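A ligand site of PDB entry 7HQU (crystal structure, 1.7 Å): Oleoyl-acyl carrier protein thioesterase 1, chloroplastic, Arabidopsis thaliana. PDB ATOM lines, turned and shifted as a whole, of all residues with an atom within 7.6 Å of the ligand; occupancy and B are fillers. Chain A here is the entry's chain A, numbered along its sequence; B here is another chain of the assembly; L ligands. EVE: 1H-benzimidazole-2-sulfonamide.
O1 of the ligand sits close to OE1 of Gln 230 (3.3 Å).
The side-chain carboxylate (OE2) of Glu 205 of chain B sits close to a nitrogen (N2) of the ligand, 2.9 Å away.
N of the ligand lies within hydrogen-bond range of O of Pro 183, 3.0 Å away.
A nitrogen (N) of the ligand sits at hydrogen-bond distance from the backbone carbonyl oxygen (O) of Gln 230.
O2 of the ligand sits at hydrogen-bond distance from N of Arg 185 (2.9 Å).
The side-chain sulfur (SD) of Met 178 of chain B lies within hydrogen-bond range of the side-chain amino group (NZ) of Lys 182.
N of Arg 184 lies within hydrogen-bond range of OD2 of Asp 187 (2.8 Å).
OE1 of Glu 205 of chain B is in hydrogen-bond range of N of Arg 185 (2.9 Å).
NH2 of Arg 185 lies within hydrogen-bond range of O of Ile 207 of chain B, 2.9 Å away.
The side-chain amide oxygen of Gln 209 of chain B lies within hydrogen-bond range of the guanidinium group of Arg 185 (2.9 Å).
NE2 of Gln 230 lies within hydrogen-bond range of O of Gln 192, 2.9 Å away.
The backbone carbonyl oxygen of Leu 204 of chain B is in hydrogen-bond range of the guanidinium group of Arg 185 (2.9 Å).
An oxygen (O2) of the ligand lies close to the backbone carbonyl oxygen (O) of Arg 184, 3.2 Å away.
Merely in contact with the ligand: Leu 188, Met 178 of chain B, Ile 207 of chain B and Gln 209 of chain B.
Hydrophobic or aromatic side chains within 4 Å of the ligand: Pro 183, Leu 188 and Met 178 of chain B.
Nine residues have an atom within 4 Å of the ligand: Pro 183, Arg 184, Arg 185, Leu 188, Gln 230, Met 178 of chain B, Glu 205 of chain B, Ile 207 of chain B and Gln 209 of chain B.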
ATOM      1  N   LYS A 182     -15.956   1.128   1.890  1.00  0.00           N
ATOM      2  CA  LYS A 182     -15.653   1.108   3.333  1.00  0.00           C
ATOM      3  C   LYS A 182     -15.669  -0.292   3.902  1.00  0.00           C
ATOM      4  O   LYS A 182     -16.468  -1.129   3.487  1.00  0.00           O
ATOM      5  CB  LYS A 182     -16.531   2.054   4.136  1.00  0.00           C
ATOM      6  CG  LYS A 182     -18.006   1.755   4.076  1.00  0.00           C
ATOM      7  CD  LYS A 182     -18.792   2.935   4.660  1.00  0.00           C
ATOM      8  CE  LYS A 182     -20.252   2.594   4.859  1.00  0.00           C
ATOM      9  NZ  LYS A 182     -21.028   3.781   5.307  1.00  0.00           N
ATOM     10  N   PRO A 183     -14.764  -0.587   4.849  1.00  0.00           N
ATOM     11  CA  PRO A 183     -14.726  -1.930   5.425  1.00  0.00           C
ATOM     12  C   PRO A 183     -15.892  -2.240   6.383  1.00  0.00           C
ATOM     13  O   PRO A 183     -16.384  -1.352   7.081  1.00  0.00           O
ATOM     14  CB  PRO A 183     -13.394  -1.933   6.196  1.00  0.00           C
ATOM     15  CG  PRO A 183     -13.212  -0.529   6.604  1.00  0.00           C
ATOM     16  CD  PRO A 183     -13.725   0.288   5.443  1.00  0.00           C
ATOM     17  N   ARG A 184     -16.326  -3.496   6.396  1.00  0.00           N
ATOM     18  CA  ARG A 184     -17.304  -3.944   7.366  1.00  0.00           C
ATOM     19  C   ARG A 184     -16.547  -4.951   8.309  1.00  0.00           C
ATOM     20  O   ARG A 184     -15.350  -5.204   8.093  1.00  0.00           O
ATOM     21  CB  ARG A 184     -18.579  -4.538   6.710  1.00  0.00           C
ATOM     22  CG  ARG A 184     -18.339  -5.697   5.750  1.00  0.00           C
ATOM     23  CD  ARG A 184     -19.663  -6.033   5.068  1.00  0.00           C
ATOM     24  NE  ARG A 184     -19.547  -7.131   4.088  1.00  0.00           N
ATOM     25  CZ  ARG A 184     -19.662  -8.420   4.402  1.00  0.00           C
ATOM     26  NH1 ARG A 184     -19.893  -8.797   5.651  1.00  0.00           N
ATOM     27  NH2 ARG A 184     -19.592  -9.348   3.456  1.00  0.00           N
ATOM     28  N   ARG A 185     -17.173  -5.415   9.397  1.00  0.00           N
ATOM     29  CA  ARG A 185     -16.470  -6.262  10.372  1.00  0.00           C
ATOM     30  C   ARG A 185     -15.813  -7.504   9.754  1.00  0.00           C
ATOM     31  O   ARG A 185     -14.710  -7.857  10.183  1.00  0.00           O
ATOM     32  CB  ARG A 185     -17.335  -6.624  11.573  1.00  0.00           C
ATOM     33  CG  ARG A 185     -17.597  -5.415  12.459  1.00  0.00           C
ATOM     34  CD  ARG A 185     -17.978  -5.819  13.872  1.00  0.00           C
ATOM     35  NE  ARG A 185     -18.444  -4.675  14.619  1.00  0.00           N
ATOM     36  CZ  ARG A 185     -19.711  -4.283  14.701  1.00  0.00           C
ATOM     37  NH1 ARG A 185     -20.669  -4.994  14.115  1.00  0.00           N
ATOM     38  NH2 ARG A 185     -20.042  -3.200  15.381  1.00  0.00           N
ATOM     39  N   ALA A 186     -16.408  -8.114   8.702  1.00  0.00           N
ATOM     40  CA  ALA A 186     -15.786  -9.262   8.035  1.00  0.00           C
ATOM     41  C   ALA A 186     -14.458  -8.906   7.348  1.00  0.00           C
ATOM     42  O   ALA A 186     -13.646  -9.786   7.124  1.00  0.00           O
ATOM     43  CB  ALA A 186     -16.740  -9.922   7.052  1.00  0.00           C
ATOM     44  N   ASP A 187     -14.213  -7.625   7.046  1.00  0.00           N
ATOM     45  CA  ASP A 187     -12.953  -7.198   6.433  1.00  0.00           C
ATOM     46  C   ASP A 187     -11.781  -7.049   7.440  1.00  0.00           C
ATOM     47  O   ASP A 187     -10.658  -6.752   7.034  1.00  0.00           O
ATOM     48  CB  ASP A 187     -13.141  -5.830   5.747  1.00  0.00           C
ATOM     49  CG  ASP A 187     -14.052  -5.898   4.534  1.00  0.00           C
ATOM     50  OD1 ASP A 187     -13.780  -6.723   3.633  1.00  0.00           O
ATOM     51  OD2 ASP A 187     -15.049  -5.161   4.502  1.00  0.00           O
ATOM     52  N   LEU A 188     -12.057  -7.148   8.742  1.00  0.00           N
ATOM     53  CA  LEU A 188     -11.028  -6.955   9.755  1.00  0.00           C
ATOM     54  C   LEU A 188     -10.393  -8.288  10.162  1.00  0.00           C
ATOM     55  O   LEU A 188     -11.045  -9.325  10.116  1.00  0.00           O
ATOM     56  CB  LEU A 188     -11.612  -6.282  11.019  1.00  0.00           C
ATOM     57  CG  LEU A 188     -12.424  -4.997  10.804  1.00  0.00           C
ATOM     58  CD1 LEU A 188     -13.004  -4.491  12.101  1.00  0.00           C
ATOM     59  CD2 LEU A 188     -11.579  -3.919  10.081  1.00  0.00           C
ATOM     60  N   GLN A 192      -8.418  -6.314  14.765  1.00  0.00           N
ATOM     61  CA  GLN A 192      -9.294  -5.214  14.342  1.00  0.00           C
ATOM     62  C   GLN A 192      -8.651  -4.268  13.328  1.00  0.00           C
ATOM     63  O   GLN A 192      -9.087  -3.127  13.171  1.00  0.00           O
ATOM     64  CB  GLN A 192      -9.877  -4.446  15.536  1.00  0.00           C
ATOM     65  CG  GLN A 192     -10.747  -5.345  16.407  1.00  0.00           C
ATOM     66  CD  GLN A 192     -11.313  -4.609  17.595  1.00  0.00           C
ATOM     67  OE1 GLN A 192     -10.582  -4.178  18.501  1.00  0.00           O
ATOM     68  NE2 GLN A 192     -12.624  -4.470  17.640  1.00  0.00           N
ATOM     69  N   HIS A 193      -7.662  -4.754  12.595  1.00  0.00           N
ATOM     70  CA  HIS A 193      -7.040  -4.002  11.530  1.00  0.00           C
ATOM     71  C   HIS A 193      -7.617  -4.546  10.203  1.00  0.00           C
ATOM     72  O   HIS A 193      -7.961  -5.732  10.130  1.00  0.00           O
ATOM     73  CB  HIS A 193      -5.515  -4.186  11.571  1.00  0.00           C
ATOM     74  CG  HIS A 193      -4.849  -3.344  12.603  1.00  0.00           C
ATOM     75  ND1 HIS A 193      -4.272  -2.120  12.283  1.00  0.00           N
ATOM     76  CD2 HIS A 193      -4.718  -3.535  13.939  1.00  0.00           C
ATOM     77  CE1 HIS A 193      -3.813  -1.619  13.422  1.00  0.00           C
ATOM     78  NE2 HIS A 193      -4.054  -2.437  14.448  1.00  0.00           N
ATOM     79  N   VAL A 194      -7.721  -3.702   9.169  1.00  0.00           N
ATOM     80  CA  VAL A 194      -8.214  -4.154   7.868  1.00  0.00           C
ATOM     81  C   VAL A 194      -7.276  -5.259   7.300  1.00  0.00           C
ATOM     82  O   VAL A 194      -6.059  -5.065   7.279  1.00  0.00           O
ATOM     83  CB  VAL A 194      -8.447  -2.988   6.873  1.00  0.00           C
ATOM     84  CG1 VAL A 194      -8.769  -3.525   5.468  1.00  0.00           C
ATOM     85  CG2 VAL A 194      -9.549  -2.047   7.361  1.00  0.00           C
ATOM     86  N   GLN A 229      -8.143   2.839   8.171  1.00  0.00           N
ATOM     87  CA  GLN A 229      -8.693   2.625   9.515  1.00  0.00           C
ATOM     88  C   GLN A 229     -10.163   2.176   9.392  1.00  0.00           C
ATOM     89  O   GLN A 229     -10.766   2.282   8.317  1.00  0.00           O
ATOM     90  CB  GLN A 229      -8.561   3.886  10.365  1.00  0.00           C
ATOM     91  CG  GLN A 229      -7.528   3.745  11.461  1.00  0.00           C
ATOM     92  CD  GLN A 229      -6.195   4.281  11.079  1.00  0.00           C
ATOM     93  OE1 GLN A 229      -5.274   3.532  10.718  1.00  0.00           O
ATOM     94  NE2 GLN A 229      -6.063   5.601  11.164  1.00  0.00           N
ATOM     95  N   GLN A 230     -10.753   1.680  10.491  1.00  0.00           N
ATOM     96  CA  GLN A 230     -12.150   1.236  10.556  1.00  0.00           C
ATOM     97  C   GLN A 230     -13.178   2.314  10.182  1.00  0.00           C
ATOM     98  O   GLN A 230     -14.245   2.000   9.686  1.00  0.00           O
ATOM     99  CB  GLN A 230     -12.463   0.720  11.975  1.00  0.00           C
ATOM    100  CG  GLN A 230     -11.582  -0.426  12.376  1.00  0.00           C
ATOM    101  CD  GLN A 230     -11.753  -0.769  13.827  1.00  0.00           C
ATOM    102  OE1 GLN A 230     -12.855  -0.755  14.362  1.00  0.00           O
ATOM    103  NE2 GLN A 230     -10.661  -1.109  14.486  1.00  0.00           N
ATOM    104  N   ASP A 231     -12.873   3.588  10.444  1.00  0.00           N
ATOM    105  CA  ASP A 231     -13.786   4.690  10.125  1.00  0.00           C
ATOM    106  C   ASP A 231     -13.412   5.468   8.820  1.00  0.00           C
ATOM    107  O   ASP A 231     -13.977   6.534   8.541  1.00  0.00           O
ATOM    108  CB  ASP A 231     -13.950   5.617  11.340  1.00  0.00           C
ATOM    109  CG  ASP A 231     -12.685   6.360  11.740  1.00  0.00           C
ATOM    110  OD1 ASP A 231     -11.583   5.985  11.257  1.00  0.00           O
ATOM    111  OD2 ASP A 231     -12.790   7.304  12.556  1.00  0.00           O
ATOM    112  N   ASP A 232     -12.458   4.919   8.039  1.00  0.00           N
ATOM    113  CA  ASP A 232     -12.017   5.531   6.785  1.00  0.00           C
ATOM    114  C   ASP A 232     -12.896   5.083   5.579  1.00  0.00           C
ATOM    115  O   ASP A 232     -13.554   4.034   5.622  1.00  0.00           O
ATOM    116  CB  ASP A 232     -10.533   5.228   6.502  1.00  0.00           C
ATOM    117  CG  ASP A 232      -9.519   6.061   7.283  1.00  0.00           C
ATOM    118  OD1 ASP A 232      -9.860   7.192   7.694  1.00  0.00           O
ATOM    119  OD2 ASP A 232      -8.363   5.579   7.474  1.00  0.00           O
ATOM    120  N   SER B 177     -27.934   2.937  13.026  1.00  0.00           N
ATOM    121  CA  SER B 177     -27.942   2.741  11.586  1.00  0.00           C
ATOM    122  C   SER B 177     -26.539   2.697  10.974  1.00  0.00           C
ATOM    123  O   SER B 177     -25.594   3.257  11.533  1.00  0.00           O
ATOM    124  CB  SER B 177     -28.788   3.811  10.885  1.00  0.00           C
ATOM    125  OG  SER B 177     -28.094   5.049  10.814  1.00  0.00           O
ATOM    126  N   MET B 178     -26.412   2.037   9.827  1.00  0.00           N
ATOM    127  CA  MET B 178     -25.186   2.014   9.038  1.00  0.00           C
ATOM    128  C   MET B 178     -25.677   2.198   7.601  1.00  0.00           C
ATOM    129  O   MET B 178     -26.440   1.363   7.112  1.00  0.00           O
ATOM    130  CB  MET B 178     -24.405   0.689   9.204  1.00  0.00           C
ATOM    131  CG  MET B 178     -23.230   0.574   8.249  1.00  0.00           C
ATOM    132  SD  MET B 178     -22.002   1.910   8.414  1.00  0.00           S
ATOM    133  CE  MET B 178     -21.145   1.384   9.916  1.00  0.00           C
ATOM    134  N   LEU B 204     -25.517  -6.927  10.984  1.00  0.00           N
ATOM    135  CA  LEU B 204     -24.619  -6.739  12.111  1.00  0.00           C
ATOM    136  C   LEU B 204     -23.859  -5.410  12.102  1.00  0.00           C
ATOM    137  O   LEU B 204     -23.412  -4.969  13.168  1.00  0.00           O
ATOM    138  CB  LEU B 204     -23.654  -7.924  12.250  1.00  0.00           C
ATOM    139  CG  LEU B 204     -24.320  -9.281  12.532  1.00  0.00           C
ATOM    140  CD1 LEU B 204     -23.273 -10.376  12.576  1.00  0.00           C
ATOM    141  CD2 LEU B 204     -25.141  -9.257  13.807  1.00  0.00           C
ATOM    142  N   GLU B 205     -23.790  -4.738  10.932  1.00  0.00           N
ATOM    143  CA  GLU B 205     -23.110  -3.461  10.856  1.00  0.00           C
ATOM    144  C   GLU B 205     -23.791  -2.351  11.652  1.00  0.00           C
ATOM    145  O   GLU B 205     -23.125  -1.385  12.018  1.00  0.00           O
ATOM    146  CB  GLU B 205     -22.890  -3.018   9.403  1.00  0.00           C
ATOM    147  CG  GLU B 205     -21.665  -3.619   8.736  1.00  0.00           C
ATOM    148  CD  GLU B 205     -20.332  -3.355   9.417  1.00  0.00           C
ATOM    149  OE1 GLU B 205     -19.771  -4.302  10.020  1.00  0.00           O
ATOM    150  OE2 GLU B 205     -19.812  -2.226   9.308  1.00  0.00           O
ATOM    151  N   SER B 206     -25.109  -2.458  11.898  1.00  0.00           N
ATOM    152  CA  SER B 206     -25.777  -1.426  12.702  1.00  0.00           C
ATOM    153  C   SER B 206     -25.792  -1.761  14.214  1.00  0.00           C
ATOM    154  O   SER B 206     -26.330  -0.982  15.000  1.00  0.00           O
ATOM    155  CB  SER B 206     -27.157  -1.100  12.149  1.00  0.00           C
ATOM    156  OG  SER B 206     -27.961  -2.267  12.078  1.00  0.00           O
ATOM    157  N   ILE B 207     -25.140  -2.852  14.639  1.00  0.00           N
ATOM    158  CA  ILE B 207     -25.015  -3.159  16.075  1.00  0.00           C
ATOM    159  C   ILE B 207     -23.810  -2.331  16.581  1.00  0.00           C
ATOM    160  O   ILE B 207     -22.751  -2.366  15.950  1.00  0.00           O
ATOM    161  CB  ILE B 207     -24.754  -4.671  16.313  1.00  0.00           C
ATOM    162  CG1 ILE B 207     -25.988  -5.544  15.928  1.00  0.00           C
ATOM    163  CG2 ILE B 207     -24.249  -4.965  17.735  1.00  0.00           C
ATOM    164  CD1 ILE B 207     -27.128  -5.580  16.947  1.00  0.00           C
ATOM    165  N   PRO B 208     -23.950  -1.582  17.702  1.00  0.00           N
ATOM    166  CA  PRO B 208     -22.802  -0.798  18.199  1.00  0.00           C
ATOM    167  C   PRO B 208     -21.604  -1.691  18.571  1.00  0.00           C
ATOM    168  O   PRO B 208     -21.780  -2.803  19.052  1.00  0.00           O
ATOM    169  CB  PRO B 208     -23.333  -0.093  19.453  1.00  0.00           C
ATOM    170  CG  PRO B 208     -24.817  -0.196  19.370  1.00  0.00           C
ATOM    171  CD  PRO B 208     -25.133  -1.444  18.570  1.00  0.00           C
ATOM    172  N   GLN B 209     -20.390  -1.159  18.390  1.00  0.00           N
ATOM    173  CA  GLN B 209     -19.155  -1.859  18.710  1.00  0.00           C
ATOM    174  C   GLN B 209     -19.076  -2.216  20.219  1.00  0.00           C
ATOM    175  O   GLN B 209     -18.511  -3.261  20.539  1.00  0.00           O
ATOM    176  CB  GLN B 209     -17.937  -1.015  18.281  1.00  0.00           C
ATOM    177  CG  GLN B 209     -16.601  -1.766  18.373  1.00  0.00           C
ATOM    178  CD  GLN B 209     -16.571  -2.973  17.464  1.00  0.00           C
ATOM    179  OE1 GLN B 209     -16.941  -2.909  16.277  1.00  0.00           O
ATOM    180  NE2 GLN B 209     -16.144  -4.119  17.984  1.00  0.00           N
ATOM    181  N   GLU B 210     -19.691  -1.419  21.102  1.00  0.00           N
ATOM    182  CA  GLU B 210     -19.723  -1.680  22.540  1.00  0.00           C
ATOM    183  C   GLU B 210     -20.460  -2.990  22.842  1.00  0.00           C
ATOM    184  O   GLU B 210     -20.028  -3.757  23.695  1.00  0.00           O
ATOM    185  CB  GLU B 210     -20.359  -0.500  23.304  1.00  0.00           C
ATOM    186  CG  GLU B 210     -19.549   0.783  23.221  1.00  0.00           C
ATOM    187  CD  GLU B 210     -19.879   1.732  22.083  1.00  0.00           C
ATOM    188  OE1 GLU B 210     -20.528   1.311  21.109  1.00  0.00           O
ATOM    189  OE2 GLU B 210     -19.469   2.913  22.181  1.00  0.00           O
ATOM    190  N   VAL B 212     -20.753  -5.541  20.630  1.00  0.00           N
ATOM    191  CA  VAL B 212     -19.869  -6.577  20.086  1.00  0.00           C
ATOM    192  C   VAL B 212     -18.669  -6.881  21.014  1.00  0.00           C
ATOM    193  O   VAL B 212     -18.299  -8.043  21.182  1.00  0.00           O
ATOM    194  CB  VAL B 212     -19.417  -6.236  18.643  1.00  0.00           C
ATOM    195  CG1 VAL B 212     -18.426  -7.272  18.116  1.00  0.00           C
ATOM    196  CG2 VAL B 212     -20.608  -6.126  17.714  1.00  0.00           C
HETATM  197  N   EVE L   1     -15.498  -0.504   9.783  1.00  0.00           N
HETATM  198  S   EVE L   1     -15.677  -1.670  10.861  1.00  0.00           S
HETATM  199  N1  EVE L   1     -16.758  -0.638  13.139  1.00  0.00           N
HETATM  200  O1  EVE L   1     -14.516  -1.692  11.692  1.00  0.00           O
HETATM  201  C2  EVE L   1     -17.010  -1.185  11.928  1.00  0.00           C
HETATM  202  N2  EVE L   1     -18.285  -1.267  11.603  1.00  0.00           N
HETATM  203  O2  EVE L   1     -16.075  -2.854  10.178  1.00  0.00           O
HETATM  204  C4  EVE L   1     -18.368   0.226  14.892  1.00  0.00           C
HETATM  205  C5  EVE L   1     -19.717   0.391  15.111  1.00  0.00           C
HETATM  206  C6  EVE L   1     -20.667   0.009  14.165  1.00  0.00           C
HETATM  207  C7  EVE L   1     -20.289  -0.531  12.951  1.00  0.00           C
HETATM  208  C8  EVE L   1     -18.935  -0.705  12.710  1.00  0.00           C
HETATM  209  C9  EVE L   1     -17.999  -0.333  13.670  1.00  0.00           C
